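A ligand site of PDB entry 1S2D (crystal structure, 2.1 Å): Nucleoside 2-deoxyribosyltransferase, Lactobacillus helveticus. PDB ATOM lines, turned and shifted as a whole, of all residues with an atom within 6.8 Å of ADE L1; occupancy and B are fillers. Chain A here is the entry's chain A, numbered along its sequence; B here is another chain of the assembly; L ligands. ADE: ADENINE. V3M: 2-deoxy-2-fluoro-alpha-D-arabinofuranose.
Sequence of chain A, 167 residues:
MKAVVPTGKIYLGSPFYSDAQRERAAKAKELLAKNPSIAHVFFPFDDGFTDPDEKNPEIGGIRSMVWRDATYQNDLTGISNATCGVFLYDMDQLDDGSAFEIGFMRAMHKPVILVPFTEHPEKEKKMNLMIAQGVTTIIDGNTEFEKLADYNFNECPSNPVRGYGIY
CE2 of Phe 45 touches C4 of ADE L1, 3.6 Å away. Trp 67 touches ADE L1 (CZ2 to C8, 3.7 Å). Thr 71 touches ADE L1. Hydrophobic or aromatic side chains that line ADE L1: Pro 44, Phe 45 and Trp 67. The nearest printed residue that does not touch ADE L1 is Leu 129 of chain B (4.1 Å).
O of Pro 44 lies within hydrogen-bond range of N6 of ADE L1. C1 of V3M L2 is covalently linked to OE2 of Glu 101 (1.4 Å). An oxygen (O5) of V3M L2 lies within hydrogen-bond range of the side-chain hydroxyl of Tyr 17, 3.0 Å away. The side-chain amide oxygen (OD1) of Asn 128 of chain B is in hydrogen-bond range of an oxygen (O5) of V3M L2 (2.9 Å). OXT of Tyr 167 of chain B lies within hydrogen-bond range of N9 of ADE L1 (2.8 Å). The side-chain carboxylate (OD2) of Asp 75 is in hydrogen-bond range of a nitrogen (N1) of ADE L1 (2.7 Å).
The backbone carbonyl oxygen of Trp 67 is in hydrogen-bond range of the side-chain hydroxyl of Thr 71 (2.8 Å).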
ATOM      1  N   TYR A  11     -11.227 -26.613 -11.688  1.00  0.00           N
ATOM      2  CA  TYR A  11     -11.400 -26.351 -10.273  1.00  0.00           C
ATOM      3  C   TYR A  11     -11.271 -24.837 -10.280  1.00  0.00           C
ATOM      4  O   TYR A  11     -10.184 -24.298 -10.499  1.00  0.00           O
ATOM      5  CB  TYR A  11     -10.274 -26.959  -9.418  1.00  0.00           C
ATOM      6  CG  TYR A  11     -10.402 -26.610  -7.942  1.00  0.00           C
ATOM      7  CD1 TYR A  11     -11.328 -27.266  -7.134  1.00  0.00           C
ATOM      8  CD2 TYR A  11      -9.569 -25.664  -7.361  1.00  0.00           C
ATOM      9  CE1 TYR A  11     -11.420 -26.969  -5.765  1.00  0.00           C
ATOM     10  CE2 TYR A  11      -9.660 -25.364  -6.002  1.00  0.00           C
ATOM     11  CZ  TYR A  11     -10.578 -26.023  -5.205  1.00  0.00           C
ATOM     12  OH  TYR A  11     -10.610 -25.778  -3.856  1.00  0.00           O
ATOM     13  N   TYR A  17     -15.487 -13.385  -0.567  1.00  0.00           N
ATOM     14  CA  TYR A  17     -15.676 -12.551   0.608  1.00  0.00           C
ATOM     15  C   TYR A  17     -16.070 -11.094   0.379  1.00  0.00           C
ATOM     16  O   TYR A  17     -16.366 -10.372   1.333  1.00  0.00           O
ATOM     17  CB  TYR A  17     -14.412 -12.691   1.470  1.00  0.00           C
ATOM     18  CG  TYR A  17     -13.934 -14.147   1.561  1.00  0.00           C
ATOM     19  CD1 TYR A  17     -14.805 -15.161   1.983  1.00  0.00           C
ATOM     20  CD2 TYR A  17     -12.650 -14.528   1.157  1.00  0.00           C
ATOM     21  CE1 TYR A  17     -14.412 -16.498   1.997  1.00  0.00           C
ATOM     22  CE2 TYR A  17     -12.240 -15.893   1.174  1.00  0.00           C
ATOM     23  CZ  TYR A  17     -13.137 -16.856   1.588  1.00  0.00           C
ATOM     24  OH  TYR A  17     -12.778 -18.195   1.640  1.00  0.00           O
ATOM     25  N   PHE A  43     -16.999 -25.266  -8.656  1.00  0.00           N
ATOM     26  CA  PHE A  43     -16.855 -24.058  -7.862  1.00  0.00           C
ATOM     27  C   PHE A  43     -17.235 -24.417  -6.432  1.00  0.00           C
ATOM     28  O   PHE A  43     -18.399 -24.680  -6.127  1.00  0.00           O
ATOM     29  CB  PHE A  43     -17.757 -22.935  -8.374  1.00  0.00           C
ATOM     30  CG  PHE A  43     -17.474 -21.590  -7.746  1.00  0.00           C
ATOM     31  CD1 PHE A  43     -16.199 -21.038  -7.819  1.00  0.00           C
ATOM     32  CD2 PHE A  43     -18.463 -20.895  -7.064  1.00  0.00           C
ATOM     33  CE1 PHE A  43     -15.916 -19.807  -7.235  1.00  0.00           C
ATOM     34  CE2 PHE A  43     -18.203 -19.663  -6.472  1.00  0.00           C
ATOM     35  CZ  PHE A  43     -16.920 -19.114  -6.555  1.00  0.00           C
ATOM     36  N   PRO A  44     -16.245 -24.429  -5.527  1.00  0.00           N
ATOM     37  CA  PRO A  44     -16.411 -24.762  -4.112  1.00  0.00           C
ATOM     38  C   PRO A  44     -17.539 -24.088  -3.334  1.00  0.00           C
ATOM     39  O   PRO A  44     -18.128 -24.717  -2.445  1.00  0.00           O
ATOM     40  CB  PRO A  44     -15.040 -24.465  -3.518  1.00  0.00           C
ATOM     41  CG  PRO A  44     -14.426 -23.477  -4.475  1.00  0.00           C
ATOM     42  CD  PRO A  44     -14.853 -24.024  -5.800  1.00  0.00           C
ATOM     43  N   PHE A  45     -17.868 -22.849  -3.674  1.00  0.00           N
ATOM     44  CA  PHE A  45     -18.934 -22.142  -2.975  1.00  0.00           C
ATOM     45  C   PHE A  45     -20.371 -22.472  -3.417  1.00  0.00           C
ATOM     46  O   PHE A  45     -21.320 -22.002  -2.809  1.00  0.00           O
ATOM     47  CB  PHE A  45     -18.669 -20.631  -2.969  1.00  0.00           C
ATOM     48  CG  PHE A  45     -17.444 -20.242  -2.183  1.00  0.00           C
ATOM     49  CD1 PHE A  45     -16.216 -20.056  -2.831  1.00  0.00           C
ATOM     50  CD2 PHE A  45     -17.501 -20.105  -0.806  1.00  0.00           C
ATOM     51  CE1 PHE A  45     -15.073 -19.755  -2.100  1.00  0.00           C
ATOM     52  CE2 PHE A  45     -16.358 -19.807  -0.066  1.00  0.00           C
ATOM     53  CZ  PHE A  45     -15.137 -19.629  -0.717  1.00  0.00           C
ATOM     54  N   ASP A  46     -20.511 -23.285  -4.469  1.00  0.00           N
ATOM     55  CA  ASP A  46     -21.830 -23.703  -4.948  1.00  0.00           C
ATOM     56  C   ASP A  46     -22.368 -24.804  -4.017  1.00  0.00           C
ATOM     57  O   ASP A  46     -23.521 -24.747  -3.573  1.00  0.00           O
ATOM     58  CB  ASP A  46     -21.760 -24.262  -6.377  1.00  0.00           C
ATOM     59  CG  ASP A  46     -21.607 -23.176  -7.431  1.00  0.00           C
ATOM     60  OD1 ASP A  46     -21.690 -21.986  -7.083  1.00  0.00           O
ATOM     61  OD2 ASP A  46     -21.396 -23.530  -8.607  1.00  0.00           O
ATOM     62  N   GLY A  48     -23.002 -26.609  -0.844  1.00  0.00           N
ATOM     63  CA  GLY A  48     -22.524 -26.655   0.528  1.00  0.00           C
ATOM     64  C   GLY A  48     -23.043 -27.832   1.343  1.00  0.00           C
ATOM     65  O   GLY A  48     -24.080 -28.414   1.010  1.00  0.00           O
ATOM     66  N   ILE A  59     -21.502 -17.635   9.004  1.00  0.00           N
ATOM     67  CA  ILE A  59     -20.221 -17.540   8.313  1.00  0.00           C
ATOM     68  C   ILE A  59     -19.274 -16.703   9.165  1.00  0.00           C
ATOM     69  O   ILE A  59     -19.656 -15.650   9.686  1.00  0.00           O
ATOM     70  CB  ILE A  59     -20.396 -16.892   6.919  1.00  0.00           C
ATOM     71  CG1 ILE A  59     -21.525 -17.601   6.161  1.00  0.00           C
ATOM     72  CG2 ILE A  59     -19.093 -16.972   6.125  1.00  0.00           C
ATOM     73  CD1 ILE A  59     -21.844 -17.020   4.786  1.00  0.00           C
ATOM     74  N   ARG A  63     -17.564 -23.073  13.642  1.00  0.00           N
ATOM     75  CA  ARG A  63     -18.270 -24.130  12.924  1.00  0.00           C
ATOM     76  C   ARG A  63     -17.956 -25.491  13.552  1.00  0.00           C
ATOM     77  O   ARG A  63     -16.897 -25.663  14.144  1.00  0.00           O
ATOM     78  CB  ARG A  63     -17.839 -24.124  11.457  1.00  0.00           C
ATOM     79  CG  ARG A  63     -17.996 -22.770  10.737  1.00  0.00           C
ATOM     80  CD  ARG A  63     -19.435 -22.267  10.775  1.00  0.00           C
ATOM     81  NE  ARG A  63     -20.399 -23.263  10.314  1.00  0.00           N
ATOM     82  CZ  ARG A  63     -20.914 -23.309   9.089  1.00  0.00           C
ATOM     83  NH1 ARG A  63     -20.545 -22.413   8.175  1.00  0.00           N
ATOM     84  NH2 ARG A  63     -21.806 -24.248   8.788  1.00  0.00           N
ATOM     85  N   TRP A  67     -18.630 -30.193  10.028  1.00  0.00           N
ATOM     86  CA  TRP A  67     -18.855 -29.313   8.887  1.00  0.00           C
ATOM     87  C   TRP A  67     -17.517 -28.960   8.268  1.00  0.00           C
ATOM     88  O   TRP A  67     -17.396 -28.860   7.041  1.00  0.00           O
ATOM     89  CB  TRP A  67     -19.570 -28.013   9.283  1.00  0.00           C
ATOM     90  CG  TRP A  67     -19.797 -27.046   8.126  1.00  0.00           C
ATOM     91  CD1 TRP A  67     -20.869 -27.019   7.280  1.00  0.00           C
ATOM     92  CD2 TRP A  67     -18.912 -26.006   7.671  1.00  0.00           C
ATOM     93  NE1 TRP A  67     -20.715 -26.039   6.330  1.00  0.00           N
ATOM     94  CE2 TRP A  67     -19.527 -25.398   6.549  1.00  0.00           C
ATOM     95  CE3 TRP A  67     -17.665 -25.526   8.098  1.00  0.00           C
ATOM     96  CZ2 TRP A  67     -18.928 -24.335   5.843  1.00  0.00           C
ATOM     97  CZ3 TRP A  67     -17.074 -24.477   7.409  1.00  0.00           C
ATOM     98  CH2 TRP A  67     -17.707 -23.895   6.287  1.00  0.00           C
ATOM     99  N   THR A  71     -16.579 -29.944   4.476  1.00  0.00           N
ATOM    100  CA  THR A  71     -16.336 -28.840   3.540  1.00  0.00           C
ATOM    101  C   THR A  71     -14.910 -28.833   3.036  1.00  0.00           C
ATOM    102  O   THR A  71     -14.669 -28.588   1.843  1.00  0.00           O
ATOM    103  CB  THR A  71     -16.695 -27.478   4.166  1.00  0.00           C
ATOM    104  OG1 THR A  71     -18.018 -27.537   4.707  1.00  0.00           O
ATOM    105  CG2 THR A  71     -16.644 -26.382   3.116  1.00  0.00           C
ATOM    106  N   TYR A  72     -13.960 -29.090   3.938  1.00  0.00           N
ATOM    107  CA  TYR A  72     -12.551 -29.127   3.555  1.00  0.00           C
ATOM    108  C   TYR A  72     -12.353 -30.252   2.545  1.00  0.00           C
ATOM    109  O   TYR A  72     -11.672 -30.078   1.528  1.00  0.00           O
ATOM    110  CB  TYR A  72     -11.667 -29.358   4.773  1.00  0.00           C
ATOM    111  CG  TYR A  72     -10.203 -29.553   4.452  1.00  0.00           C
ATOM    112  CD1 TYR A  72      -9.429 -28.480   3.997  1.00  0.00           C
ATOM    113  CD2 TYR A  72      -9.584 -30.779   4.656  1.00  0.00           C
ATOM    114  CE1 TYR A  72      -8.070 -28.631   3.774  1.00  0.00           C
ATOM    115  CE2 TYR A  72      -8.214 -30.949   4.429  1.00  0.00           C
ATOM    116  CZ  TYR A  72      -7.458 -29.867   3.985  1.00  0.00           C
ATOM    117  OH  TYR A  72      -6.105 -29.996   3.789  1.00  0.00           O
ATOM    118  N   ASN A  74     -14.616 -31.517   0.593  1.00  0.00           N
ATOM    119  CA  ASN A  74     -15.300 -31.144  -0.637  1.00  0.00           C
ATOM    120  C   ASN A  74     -14.368 -30.313  -1.507  1.00  0.00           C
ATOM    121  O   ASN A  74     -14.350 -30.480  -2.719  1.00  0.00           O
ATOM    122  CB  ASN A  74     -16.582 -30.362  -0.333  1.00  0.00           C
ATOM    123  CG  ASN A  74     -17.776 -31.262  -0.190  1.00  0.00           C
ATOM    124  OD1 ASN A  74     -17.776 -32.388  -0.684  1.00  0.00           O
ATOM    125  ND2 ASN A  74     -18.821 -30.781   0.475  1.00  0.00           N
ATOM    126  N   ASP A  75     -13.599 -29.431  -0.868  1.00  0.00           N
ATOM    127  CA  ASP A  75     -12.644 -28.594  -1.587  1.00  0.00           C
ATOM    128  C   ASP A  75     -11.504 -29.442  -2.164  1.00  0.00           C
ATOM    129  O   ASP A  75     -11.113 -29.236  -3.313  1.00  0.00           O
ATOM    130  CB  ASP A  75     -12.094 -27.477  -0.677  1.00  0.00           C
ATOM    131  CG  ASP A  75     -13.157 -26.452  -0.312  1.00  0.00           C
ATOM    132  OD1 ASP A  75     -14.228 -26.406  -0.963  1.00  0.00           O
ATOM    133  OD2 ASP A  75     -12.942 -25.673   0.644  1.00  0.00           O
ATOM    134  N   GLU A 101      -4.497 -24.001  -1.990  1.00  0.00           N
ATOM    135  CA  GLU A 101      -5.022 -24.813  -3.068  1.00  0.00           C
ATOM    136  C   GLU A 101      -4.105 -24.859  -4.296  1.00  0.00           C
ATOM    137  O   GLU A 101      -3.952 -25.924  -4.915  1.00  0.00           O
ATOM    138  CB  GLU A 101      -6.432 -24.359  -3.420  1.00  0.00           C
ATOM    139  CG  GLU A 101      -7.400 -24.550  -2.226  1.00  0.00           C
ATOM    140  CD  GLU A 101      -8.689 -23.764  -2.309  1.00  0.00           C
ATOM    141  OE1 GLU A 101      -8.815 -22.950  -3.261  1.00  0.00           O
ATOM    142  OE2 GLU A 101      -9.550 -24.067  -1.421  1.00  0.00           O
ATOM    143  N   ASN B 128      -8.926 -19.062   7.471  1.00  0.00           N
ATOM    144  CA  ASN B 128      -9.439 -19.660   6.249  1.00  0.00           C
ATOM    145  C   ASN B 128      -9.540 -21.160   6.514  1.00  0.00           C
ATOM    146  O   ASN B 128      -8.660 -21.743   7.133  1.00  0.00           O
ATOM    147  CB  ASN B 128      -8.477 -19.393   5.077  1.00  0.00           C
ATOM    148  CG  ASN B 128      -9.072 -19.791   3.729  1.00  0.00           C
ATOM    149  OD1 ASN B 128      -9.546 -18.943   2.974  1.00  0.00           O
ATOM    150  ND2 ASN B 128      -9.017 -21.080   3.421  1.00  0.00           N
ATOM    151  N   LEU B 129     -10.626 -21.771   6.041  1.00  0.00           N
ATOM    152  CA  LEU B 129     -10.837 -23.210   6.261  1.00  0.00           C
ATOM    153  C   LEU B 129      -9.675 -24.083   5.814  1.00  0.00           C
ATOM    154  O   LEU B 129      -9.329 -25.046   6.501  1.00  0.00           O
ATOM    155  CB  LEU B 129     -12.139 -23.672   5.583  1.00  0.00           C
ATOM    156  CG  LEU B 129     -12.500 -25.165   5.689  1.00  0.00           C
ATOM    157  CD1 LEU B 129     -12.785 -25.548   7.130  1.00  0.00           C
ATOM    158  CD2 LEU B 129     -13.694 -25.476   4.804  1.00  0.00           C
ATOM    159  N   MET B 130      -9.064 -23.761   4.679  1.00  0.00           N
ATOM    160  CA  MET B 130      -7.951 -24.568   4.153  1.00  0.00           C
ATOM    161  C   MET B 130      -6.783 -24.638   5.131  1.00  0.00           C
ATOM    162  O   MET B 130      -6.129 -25.679   5.257  1.00  0.00           O
ATOM    163  CB  MET B 130      -7.481 -24.045   2.802  1.00  0.00           C
ATOM    164  CG  MET B 130      -8.577 -23.999   1.739  1.00  0.00           C
ATOM    165  SD  MET B 130      -9.622 -25.487   1.679  1.00  0.00           S
ATOM    166  CE  MET B 130      -8.539 -26.630   0.850  1.00  0.00           C
ATOM    167  N   ILE B 166     -14.544 -19.584  11.173  1.00  0.00           N
ATOM    168  CA  ILE B 166     -14.188 -20.051   9.830  1.00  0.00           C
ATOM    169  C   ILE B 166     -15.054 -19.438   8.749  1.00  0.00           C
ATOM    170  O   ILE B 166     -16.266 -19.408   8.855  1.00  0.00           O
ATOM    171  CB  ILE B 166     -14.215 -21.597   9.752  1.00  0.00           C
ATOM    172  CG1 ILE B 166     -13.072 -22.164  10.601  1.00  0.00           C
ATOM    173  CG2 ILE B 166     -14.082 -22.065   8.304  1.00  0.00           C
ATOM    174  CD1 ILE B 166     -12.743 -23.611  10.334  1.00  0.00           C
ATOM    175  N   TYR B 167     -14.386 -18.931   7.705  1.00  0.00           N
ATOM    176  CA  TYR B 167     -15.081 -18.313   6.578  1.00  0.00           C
ATOM    177  C   TYR B 167     -14.837 -19.045   5.261  1.00  0.00           C
ATOM    178  O   TYR B 167     -13.768 -19.685   5.116  1.00  0.00           O
ATOM    179  CB  TYR B 167     -14.685 -16.838   6.449  1.00  0.00           C
ATOM    180  CG  TYR B 167     -13.203 -16.579   6.350  1.00  0.00           C
ATOM    181  CD1 TYR B 167     -12.578 -16.461   5.102  1.00  0.00           C
ATOM    182  CD2 TYR B 167     -12.419 -16.417   7.488  1.00  0.00           C
ATOM    183  CE1 TYR B 167     -11.212 -16.192   5.005  1.00  0.00           C
ATOM    184  CE2 TYR B 167     -11.056 -16.138   7.405  1.00  0.00           C
ATOM    185  CZ  TYR B 167     -10.457 -16.037   6.149  1.00  0.00           C
ATOM    186  OH  TYR B 167      -9.112 -15.780   6.058  1.00  0.00           O
ATOM    187  OXT TYR B 167     -15.724 -18.964   4.385  1.00  0.00           O
HETATM  188  N9  ADE L   1     -16.974 -21.364   3.529  1.00  0.00           N
HETATM  189  C8  ADE L   1     -18.152 -21.910   3.141  1.00  0.00           C
HETATM  190  N7  ADE L   1     -18.063 -22.818   2.196  1.00  0.00           N
HETATM  191  C5  ADE L   1     -16.671 -22.869   1.954  1.00  0.00           C
HETATM  192  C6  ADE L   1     -15.872 -23.636   1.044  1.00  0.00           C
HETATM  193  N6  ADE L   1     -16.404 -24.534   0.212  1.00  0.00           N
HETATM  194  N1  ADE L   1     -14.502 -23.448   1.050  1.00  0.00           N
HETATM  195  C2  ADE L   1     -13.945 -22.535   1.899  1.00  0.00           C
HETATM  196  N3  ADE L   1     -14.620 -21.764   2.790  1.00  0.00           N
HETATM  197  C4  ADE L   1     -15.985 -21.976   2.767  1.00  0.00           C
HETATM  198  O5  V3M L   2     -10.372 -19.216   0.206  1.00  0.00           O
HETATM  199  C5  V3M L   2     -11.327 -19.955  -0.576  1.00  0.00           C
HETATM  200  C4  V3M L   2     -10.615 -20.806  -1.613  1.00  0.00           C
HETATM  201  O4  V3M L   2      -9.793 -21.868  -1.100  1.00  0.00           O
HETATM  202  C1  V3M L   2     -10.499 -23.117  -1.089  1.00  0.00           C
HETATM  203  C2  V3M L   2     -11.531 -23.008  -2.200  1.00  0.00           C
HETATM  204  F2  V3M L   2     -12.781 -23.386  -1.727  1.00  0.00           F
HETATM  205  C3  V3M L   2     -11.526 -21.525  -2.542  1.00  0.00           C
HETATM  206  O3  V3M L   2     -11.025 -21.443  -3.686  1.00  0.00           O
